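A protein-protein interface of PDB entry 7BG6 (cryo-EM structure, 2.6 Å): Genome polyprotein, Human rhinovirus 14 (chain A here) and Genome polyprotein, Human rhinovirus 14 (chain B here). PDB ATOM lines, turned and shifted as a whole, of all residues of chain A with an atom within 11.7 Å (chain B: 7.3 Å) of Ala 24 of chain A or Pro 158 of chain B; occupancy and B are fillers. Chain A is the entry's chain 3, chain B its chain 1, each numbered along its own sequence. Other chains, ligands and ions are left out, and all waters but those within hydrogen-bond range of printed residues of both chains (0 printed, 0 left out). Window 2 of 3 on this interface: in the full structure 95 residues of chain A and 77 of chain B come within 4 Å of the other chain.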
ATOM      1  N   GLN A  20     -17.386 -44.074   8.486  1.00  0.00           N
ATOM      2  CA  GLN A  20     -16.858 -43.203   7.449  1.00  0.00           C
ATOM      3  C   GLN A  20     -17.263 -41.766   7.764  1.00  0.00           C
ATOM      4  O   GLN A  20     -18.251 -41.535   8.459  1.00  0.00           O
ATOM      5  CB  GLN A  20     -17.392 -43.614   6.076  1.00  0.00           C
ATOM      6  CG  GLN A  20     -16.968 -45.008   5.632  1.00  0.00           C
ATOM      7  CD  GLN A  20     -17.498 -45.357   4.262  1.00  0.00           C
ATOM      8  OE1 GLN A  20     -17.410 -44.573   3.320  1.00  0.00           O
ATOM      9  NE2 GLN A  20     -18.052 -46.553   4.139  1.00  0.00           N
ATOM     10  N   SER A  21     -16.487 -40.811   7.241  1.00  0.00           N
ATOM     11  CA  SER A  21     -16.731 -39.394   7.460  1.00  0.00           C
ATOM     12  C   SER A  21     -16.194 -38.591   6.278  1.00  0.00           C
ATOM     13  O   SER A  21     -15.276 -39.041   5.596  1.00  0.00           O
ATOM     14  CB  SER A  21     -16.119 -38.938   8.762  1.00  0.00           C
ATOM     15  OG  SER A  21     -14.729 -39.222   8.795  1.00  0.00           O
ATOM     16  N   PRO A  22     -16.745 -37.387   5.990  1.00  0.00           N
ATOM     17  CA  PRO A  22     -16.233 -36.550   4.903  1.00  0.00           C
ATOM     18  C   PRO A  22     -14.854 -35.979   5.223  1.00  0.00           C
ATOM     19  O   PRO A  22     -14.622 -35.487   6.327  1.00  0.00           O
ATOM     20  CB  PRO A  22     -17.277 -35.430   4.787  1.00  0.00           C
ATOM     21  CG  PRO A  22     -17.900 -35.351   6.165  1.00  0.00           C
ATOM     22  CD  PRO A  22     -17.893 -36.776   6.680  1.00  0.00           C
ATOM     23  N   SER A  23     -13.946 -36.061   4.245  1.00  0.00           N
ATOM     24  CA  SER A  23     -12.606 -35.518   4.391  1.00  0.00           C
ATOM     25  C   SER A  23     -12.639 -34.004   4.196  1.00  0.00           C
ATOM     26  O   SER A  23     -13.282 -33.505   3.274  1.00  0.00           O
ATOM     27  CB  SER A  23     -11.639 -36.184   3.448  1.00  0.00           C
ATOM     28  OG  SER A  23     -10.376 -35.534   3.467  1.00  0.00           O
ATOM     29  N   ALA A  24     -11.930 -33.293   5.080  1.00  0.00           N
ATOM     30  CA  ALA A  24     -11.895 -31.839   5.081  1.00  0.00           C
ATOM     31  C   ALA A  24     -10.800 -31.336   4.143  1.00  0.00           C
ATOM     32  O   ALA A  24     -10.709 -30.138   3.881  1.00  0.00           O
ATOM     33  CB  ALA A  24     -11.697 -31.333   6.489  1.00  0.00           C
ATOM     34  N   LEU A  25      -9.970 -32.262   3.651  1.00  0.00           N
ATOM     35  CA  LEU A  25      -8.931 -31.941   2.684  1.00  0.00           C
ATOM     36  C   LEU A  25      -9.082 -32.856   1.471  1.00  0.00           C
ATOM     37  O   LEU A  25      -8.402 -33.876   1.373  1.00  0.00           O
ATOM     38  CB  LEU A  25      -7.557 -32.106   3.341  1.00  0.00           C
ATOM     39  CG  LEU A  25      -7.272 -31.212   4.550  1.00  0.00           C
ATOM     40  CD1 LEU A  25      -5.976 -31.620   5.225  1.00  0.00           C
ATOM     41  CD2 LEU A  25      -7.217 -29.746   4.148  1.00  0.00           C
ATOM     42  N   PRO A  26      -9.983 -32.526   0.513  1.00  0.00           N
ATOM     43  CA  PRO A  26     -10.205 -33.376  -0.658  1.00  0.00           C
ATOM     44  C   PRO A  26      -9.053 -33.291  -1.656  1.00  0.00           C
ATOM     45  O   PRO A  26      -8.480 -32.221  -1.860  1.00  0.00           O
ATOM     46  CB  PRO A  26     -11.498 -32.813  -1.268  1.00  0.00           C
ATOM     47  CG  PRO A  26     -11.510 -31.357  -0.849  1.00  0.00           C
ATOM     48  CD  PRO A  26     -10.832 -31.323   0.506  1.00  0.00           C
ATOM     49  N   ASN A  27      -8.718 -34.446  -2.247  1.00  0.00           N
ATOM     50  CA  ASN A  27      -7.715 -34.566  -3.296  1.00  0.00           C
ATOM     51  C   ASN A  27      -6.320 -34.281  -2.744  1.00  0.00           C
ATOM     52  O   ASN A  27      -5.368 -34.140  -3.508  1.00  0.00           O
ATOM     53  CB  ASN A  27      -8.046 -33.702  -4.519  1.00  0.00           C
ATOM     54  CG  ASN A  27      -9.427 -33.964  -5.083  1.00  0.00           C
ATOM     55  OD1 ASN A  27      -9.744 -35.087  -5.469  1.00  0.00           O
ATOM     56  ND2 ASN A  27     -10.252 -32.932  -5.143  1.00  0.00           N
ATOM     57  N   TYR A  28      -6.207 -34.200  -1.412  1.00  0.00           N
ATOM     58  CA  TYR A  28      -4.922 -33.996  -0.765  1.00  0.00           C
ATOM     59  C   TYR A  28      -4.116 -35.290  -0.829  1.00  0.00           C
ATOM     60  O   TYR A  28      -4.632 -36.364  -0.523  1.00  0.00           O
ATOM     61  CB  TYR A  28      -5.105 -33.511   0.677  1.00  0.00           C
ATOM     62  CG  TYR A  28      -3.841 -33.483   1.502  1.00  0.00           C
ATOM     63  CD1 TYR A  28      -3.092 -32.324   1.628  1.00  0.00           C
ATOM     64  CD2 TYR A  28      -3.389 -34.620   2.154  1.00  0.00           C
ATOM     65  CE1 TYR A  28      -1.927 -32.293   2.381  1.00  0.00           C
ATOM     66  CE2 TYR A  28      -2.228 -34.607   2.912  1.00  0.00           C
ATOM     67  CZ  TYR A  28      -1.495 -33.439   3.024  1.00  0.00           C
ATOM     68  OH  TYR A  28      -0.350 -33.418   3.768  1.00  0.00           O
ATOM     69  N   GLU A  29      -2.847 -35.164  -1.232  1.00  0.00           N
ATOM     70  CA  GLU A  29      -1.921 -36.282  -1.268  1.00  0.00           C
ATOM     71  C   GLU A  29      -1.106 -36.285   0.023  1.00  0.00           C
ATOM     72  O   GLU A  29      -0.385 -35.328   0.300  1.00  0.00           O
ATOM     73  CB  GLU A  29      -1.029 -36.188  -2.510  1.00  0.00           C
ATOM     74  CG  GLU A  29      -0.066 -37.354  -2.674  1.00  0.00           C
ATOM     75  CD  GLU A  29       1.218 -37.286  -1.861  1.00  0.00           C
ATOM     76  OE1 GLU A  29       1.633 -36.170  -1.488  1.00  0.00           O
ATOM     77  OE2 GLU A  29       1.803 -38.355  -1.603  1.00  0.00           O
ATOM     78  N   GLN B 133     -18.958 -21.904  13.690  1.00  0.00           N
ATOM     79  CA  GLN B 133     -18.061 -22.165  12.578  1.00  0.00           C
ATOM     80  C   GLN B 133     -16.713 -22.628  13.123  1.00  0.00           C
ATOM     81  O   GLN B 133     -16.073 -21.918  13.897  1.00  0.00           O
ATOM     82  CB  GLN B 133     -17.890 -20.936  11.683  1.00  0.00           C
ATOM     83  CG  GLN B 133     -16.942 -21.178  10.515  1.00  0.00           C
ATOM     84  CD  GLN B 133     -16.718 -19.971   9.636  1.00  0.00           C
ATOM     85  OE1 GLN B 133     -17.114 -18.854   9.959  1.00  0.00           O
ATOM     86  NE2 GLN B 133     -16.070 -20.191   8.503  1.00  0.00           N
ATOM     87  N   ALA B 134     -16.307 -23.834  12.713  1.00  0.00           N
ATOM     88  CA  ALA B 134     -14.975 -24.347  12.976  1.00  0.00           C
ATOM     89  C   ALA B 134     -14.148 -24.234  11.699  1.00  0.00           C
ATOM     90  O   ALA B 134     -14.445 -24.889  10.701  1.00  0.00           O
ATOM     91  CB  ALA B 134     -15.056 -25.771  13.469  1.00  0.00           C
ATOM     92  N   MET B 135     -13.117 -23.384  11.748  1.00  0.00           N
ATOM     93  CA  MET B 135     -12.319 -23.053  10.579  1.00  0.00           C
ATOM     94  C   MET B 135     -10.898 -23.577  10.771  1.00  0.00           C
ATOM     95  O   MET B 135     -10.242 -23.257  11.760  1.00  0.00           O
ATOM     96  CB  MET B 135     -12.289 -21.535  10.370  1.00  0.00           C
ATOM     97  CG  MET B 135     -11.549 -21.099   9.121  1.00  0.00           C
ATOM     98  SD  MET B 135     -11.538 -19.297   8.960  1.00  0.00           S
ATOM     99  CE  MET B 135     -10.258 -19.089   7.725  1.00  0.00           C
ATOM    100  N   TYR B 136     -10.445 -24.385   9.806  1.00  0.00           N
ATOM    101  CA  TYR B 136      -9.098 -24.930   9.812  1.00  0.00           C
ATOM    102  C   TYR B 136      -8.145 -23.909   9.197  1.00  0.00           C
ATOM    103  O   TYR B 136      -8.298 -23.532   8.036  1.00  0.00           O
ATOM    104  CB  TYR B 136      -9.071 -26.282   9.092  1.00  0.00           C
ATOM    105  CG  TYR B 136      -7.723 -26.957   9.037  1.00  0.00           C
ATOM    106  CD1 TYR B 136      -6.957 -26.925   7.882  1.00  0.00           C
ATOM    107  CD2 TYR B 136      -7.213 -27.633  10.136  1.00  0.00           C
ATOM    108  CE1 TYR B 136      -5.719 -27.544   7.817  1.00  0.00           C
ATOM    109  CE2 TYR B 136      -5.976 -28.257  10.088  1.00  0.00           C
ATOM    110  CZ  TYR B 136      -5.227 -28.211   8.925  1.00  0.00           C
ATOM    111  OH  TYR B 136      -4.008 -28.820   8.858  1.00  0.00           O
ATOM    112  N   VAL B 137      -7.174 -23.463  10.003  1.00  0.00           N
ATOM    113  CA  VAL B 137      -6.218 -22.446   9.596  1.00  0.00           C
ATOM    114  C   VAL B 137      -4.829 -23.082   9.540  1.00  0.00           C
ATOM    115  O   VAL B 137      -4.123 -23.127  10.547  1.00  0.00           O
ATOM    116  CB  VAL B 137      -6.255 -21.218  10.530  1.00  0.00           C
ATOM    117  CG1 VAL B 137      -5.344 -20.101  10.043  1.00  0.00           C
ATOM    118  CG2 VAL B 137      -7.670 -20.695  10.733  1.00  0.00           C
ATOM    119  N   PRO B 138      -4.401 -23.602   8.367  1.00  0.00           N
ATOM    120  CA  PRO B 138      -3.051 -24.147   8.212  1.00  0.00           C
ATOM    121  C   PRO B 138      -2.008 -23.035   8.284  1.00  0.00           C
ATOM    122  O   PRO B 138      -2.327 -21.877   8.018  1.00  0.00           O
ATOM    123  CB  PRO B 138      -3.075 -24.764   6.807  1.00  0.00           C
ATOM    124  CG  PRO B 138      -4.151 -23.992   6.076  1.00  0.00           C
ATOM    125  CD  PRO B 138      -5.192 -23.690   7.130  1.00  0.00           C
ATOM    126  N   SER B 154     -13.298 -18.244   4.179  1.00  0.00           N
ATOM    127  CA  SER B 154     -12.802 -19.596   3.969  1.00  0.00           C
ATOM    128  C   SER B 154     -12.985 -20.019   2.514  1.00  0.00           C
ATOM    129  O   SER B 154     -13.546 -21.079   2.236  1.00  0.00           O
ATOM    130  CB  SER B 154     -13.450 -20.573   4.924  1.00  0.00           C
ATOM    131  OG  SER B 154     -13.210 -20.201   6.273  1.00  0.00           O
ATOM    132  N   ALA B 155     -12.495 -19.180   1.594  1.00  0.00           N
ATOM    133  CA  ALA B 155     -12.605 -19.436   0.167  1.00  0.00           C
ATOM    134  C   ALA B 155     -11.763 -20.650  -0.220  1.00  0.00           C
ATOM    135  O   ALA B 155     -12.078 -21.339  -1.189  1.00  0.00           O
ATOM    136  CB  ALA B 155     -12.206 -18.210  -0.616  1.00  0.00           C
ATOM    137  N   SER B 156     -10.698 -20.902   0.551  1.00  0.00           N
ATOM    138  CA  SER B 156      -9.800 -22.018   0.298  1.00  0.00           C
ATOM    139  C   SER B 156      -9.597 -22.842   1.569  1.00  0.00           C
ATOM    140  O   SER B 156      -9.218 -24.010   1.494  1.00  0.00           O
ATOM    141  CB  SER B 156      -8.486 -21.543  -0.268  1.00  0.00           C
ATOM    142  OG  SER B 156      -8.693 -20.676  -1.373  1.00  0.00           O
ATOM    143  N   ASN B 157      -9.846 -22.222   2.729  1.00  0.00           N
ATOM    144  CA  ASN B 157      -9.719 -22.889   4.015  1.00  0.00           C
ATOM    145  C   ASN B 157     -10.894 -23.842   4.218  1.00  0.00           C
ATOM    146  O   ASN B 157     -12.032 -23.497   3.901  1.00  0.00           O
ATOM    147  CB  ASN B 157      -9.621 -21.892   5.175  1.00  0.00           C
ATOM    148  CG  ASN B 157      -8.252 -21.259   5.321  1.00  0.00           C
ATOM    149  OD1 ASN B 157      -8.087 -20.289   6.055  1.00  0.00           O
ATOM    150  ND2 ASN B 157      -7.261 -21.801   4.633  1.00  0.00           N
ATOM    151  N   PRO B 158     -10.654 -25.071   4.734  1.00  0.00           N
ATOM    152  CA  PRO B 158     -11.739 -25.953   5.170  1.00  0.00           C
ATOM    153  C   PRO B 158     -12.466 -25.337   6.361  1.00  0.00           C
ATOM    154  O   PRO B 158     -11.833 -24.807   7.273  1.00  0.00           O
ATOM    155  CB  PRO B 158     -11.023 -27.239   5.610  1.00  0.00           C
ATOM    156  CG  PRO B 158      -9.667 -27.168   4.941  1.00  0.00           C
ATOM    157  CD  PRO B 158      -9.330 -25.693   4.891  1.00  0.00           C
ATOM    158  N   SER B 159     -13.802 -25.408   6.331  1.00  0.00           N
ATOM    159  CA  SER B 159     -14.638 -24.830   7.369  1.00  0.00           C
ATOM    160  C   SER B 159     -15.886 -25.685   7.573  1.00  0.00           C
ATOM    161  O   SER B 159     -16.420 -26.246   6.618  1.00  0.00           O
ATOM    162  CB  SER B 159     -14.998 -23.405   7.037  1.00  0.00           C
ATOM    163  OG  SER B 159     -15.885 -22.870   8.007  1.00  0.00           O
ATOM    164  N   VAL B 160     -16.336 -25.770   8.831  1.00  0.00           N
ATOM    165  CA  VAL B 160     -17.532 -26.517   9.183  1.00  0.00           C
ATOM    166  C   VAL B 160     -18.481 -25.600   9.951  1.00  0.00           C
ATOM    167  O   VAL B 160     -18.062 -24.883  10.856  1.00  0.00           O
ATOM    168  CB  VAL B 160     -17.212 -27.786  10.002  1.00  0.00           C
ATOM    169  CG1 VAL B 160     -18.398 -28.737  10.050  1.00  0.00           C
ATOM    170  CG2 VAL B 160     -15.974 -28.509   9.495  1.00  0.00           C
ATOM    171  N   PHE B 170     -15.595 -34.768  10.696  1.00  0.00           N
ATOM    172  CA  PHE B 170     -14.867 -34.722   9.438  1.00  0.00           C
ATOM    173  C   PHE B 170     -13.538 -35.463   9.568  1.00  0.00           C
ATOM    174  O   PHE B 170     -12.891 -35.419  10.613  1.00  0.00           O
ATOM    175  CB  PHE B 170     -14.668 -33.279   8.962  1.00  0.00           C
ATOM    176  CG  PHE B 170     -13.971 -32.365   9.938  1.00  0.00           C
ATOM    177  CD1 PHE B 170     -14.701 -31.604  10.838  1.00  0.00           C
ATOM    178  CD2 PHE B 170     -12.588 -32.256   9.954  1.00  0.00           C
ATOM    179  CE1 PHE B 170     -14.064 -30.759  11.735  1.00  0.00           C
ATOM    180  CE2 PHE B 170     -11.951 -31.413  10.852  1.00  0.00           C
ATOM    181  CZ  PHE B 170     -12.690 -30.666  11.742  1.00  0.00           C
ATOM    182  N   SER B 171     -13.151 -36.135   8.479  1.00  0.00           N
ATOM    183  CA  SER B 171     -11.871 -36.814   8.389  1.00  0.00           C
ATOM    184  C   SER B 171     -10.807 -35.843   7.887  1.00  0.00           C
ATOM    185  O   SER B 171     -11.103 -34.924   7.125  1.00  0.00           O
ATOM    186  CB  SER B 171     -11.960 -38.026   7.502  1.00  0.00           C
ATOM    187  OG  SER B 171     -10.693 -38.656   7.389  1.00  0.00           O
ATOM    188  N   VAL B 172      -9.570 -36.060   8.342  1.00  0.00           N
ATOM    189  CA  VAL B 172      -8.413 -35.323   7.863  1.00  0.00           C
ATOM    190  C   VAL B 172      -7.321 -36.341   7.544  1.00  0.00           C
ATOM    191  O   VAL B 172      -6.961 -37.146   8.401  1.00  0.00           O
ATOM    192  CB  VAL B 172      -7.934 -34.276   8.891  1.00  0.00           C
ATOM    193  CG1 VAL B 172      -6.713 -33.512   8.403  1.00  0.00           C
ATOM    194  CG2 VAL B 172      -9.039 -33.308   9.290  1.00  0.00           C
ATOM    195  N   PRO B 173      -6.774 -36.352   6.306  1.00  0.00           N
ATOM    196  CA  PRO B 173      -5.669 -37.249   5.965  1.00  0.00           C
ATOM    197  C   PRO B 173      -4.422 -36.888   6.765  1.00  0.00           C
ATOM    198  O   PRO B 173      -4.391 -35.861   7.442  1.00  0.00           O
ATOM    199  CB  PRO B 173      -5.446 -37.007   4.464  1.00  0.00           C
ATOM    200  CG  PRO B 173      -6.016 -35.626   4.215  1.00  0.00           C
ATOM    201  CD  PRO B 173      -7.181 -35.502   5.175  1.00  0.00           C
ATOM    202  N   SER B 207      -4.143 -25.177  12.696  1.00  0.00           N
ATOM    203  CA  SER B 207      -4.900 -24.523  13.748  1.00  0.00           C
ATOM    204  C   SER B 207      -6.394 -24.617  13.454  1.00  0.00           C
ATOM    205  O   SER B 207      -6.796 -24.830  12.310  1.00  0.00           O
ATOM    206  CB  SER B 207      -4.456 -23.094  13.930  1.00  0.00           C
ATOM    207  OG  SER B 207      -4.902 -22.584  15.178  1.00  0.00           O
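The backbone NH (N) of Ser 171 of chain B sits close to the side-chain hydroxyl (OG) of Ser 21 of chain A.
The backbone NH (N) of Ser 171 of chain B is in hydrogen-bond range of the backbone carbonyl oxygen (O) of Pro 22 of chain A (2.7 Å).
The backbone carbonyl oxygen (O) of Ser 171 of chain B lies within hydrogen-bond range of the backbone NH (N) of Ala 24 of chain A (2.7 Å).
The backbone NH (N) of Tyr 136 of chain B is in hydrogen-bond range of the backbone carbonyl oxygen (O) of Pro 158 of chain B (2.9 Å).
The side-chain hydroxyl of Ser 23 of chain A sits close to the backbone NH of Leu 25 of chain A, at 3.3 Å.
O of Pro 22 of chain A touches CA of Phe 170 of chain B, at 3.2 Å.
Ser 23 of chain A touches Ser 171 of chain B (CA to O, 3.2 Å).
Ser 23 of chain A touches Pro 173 of chain B (OG to CD, 3.6 Å).
Ala 24 of chain A touches Pro 158 of chain B.
Ala 24 of chain A touches Phe 170 of chain B (CB to CD2, 3.7 Å).
Leu 25 of chain A touches Pro 158 of chain B.
Val 172 of chain B touches Leu 25 of chain A (CG1 to CD1, 3.8 Å).
Leu 25 of chain A touches Pro 173 of chain B.
Tyr 28 of chain A touches Pro 173 of chain B (CD2 to CG, 3.5 Å).
Of the printed residues of chain B, Ser 23 of chain A touches Ser 171 and Pro 173.
Ala 24 of chain A touches just these residues of chain B: Pro 158 (3.3 Å), Phe 170 (3.7 Å) and Ser 171 (2.7 Å).
Of the printed residues of chain B, Leu 25 of chain A touches Pro 158 (3.6 Å), Val 172 (3.8 Å) and Pro 173 (3.9 Å).
Of the printed residues of chain B, Tyr 28 of chain A touches Pro 173.
No residue of chain A comes within 4 Å of Ala 134 of chain B.
No residue of chain A comes within 4 Å of Asn 157 of chain B.
Of chain A, only Ala 24 (3.3 Å) and Leu 25 (3.6 Å) come within 4 Å of Pro 158 of chain B.
Ser 159 of chain B touches none of the printed residues of chain A.
Ser 171 of chain B touches four residues of chain A.
Val 172 of chain B touches one residue of chain A.
The nearest residue of chain B that does not touch Ala 24 of chain A is Val 172 of chain B (4.3 Å).
The nearest residue of chain A that does not touch Pro 158 of chain B is Pro 26 of chain A (6.2 Å).
Hydrophobic or aromatic side chains of chain A within 4 Å of the printed part of chain B: Ala 24, Leu 25 and Tyr 28.
Among the printed residues, no Asp or Glu carboxylate lies within 4 Å of a Lys or Arg side-chain nitrogen of the other chain.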
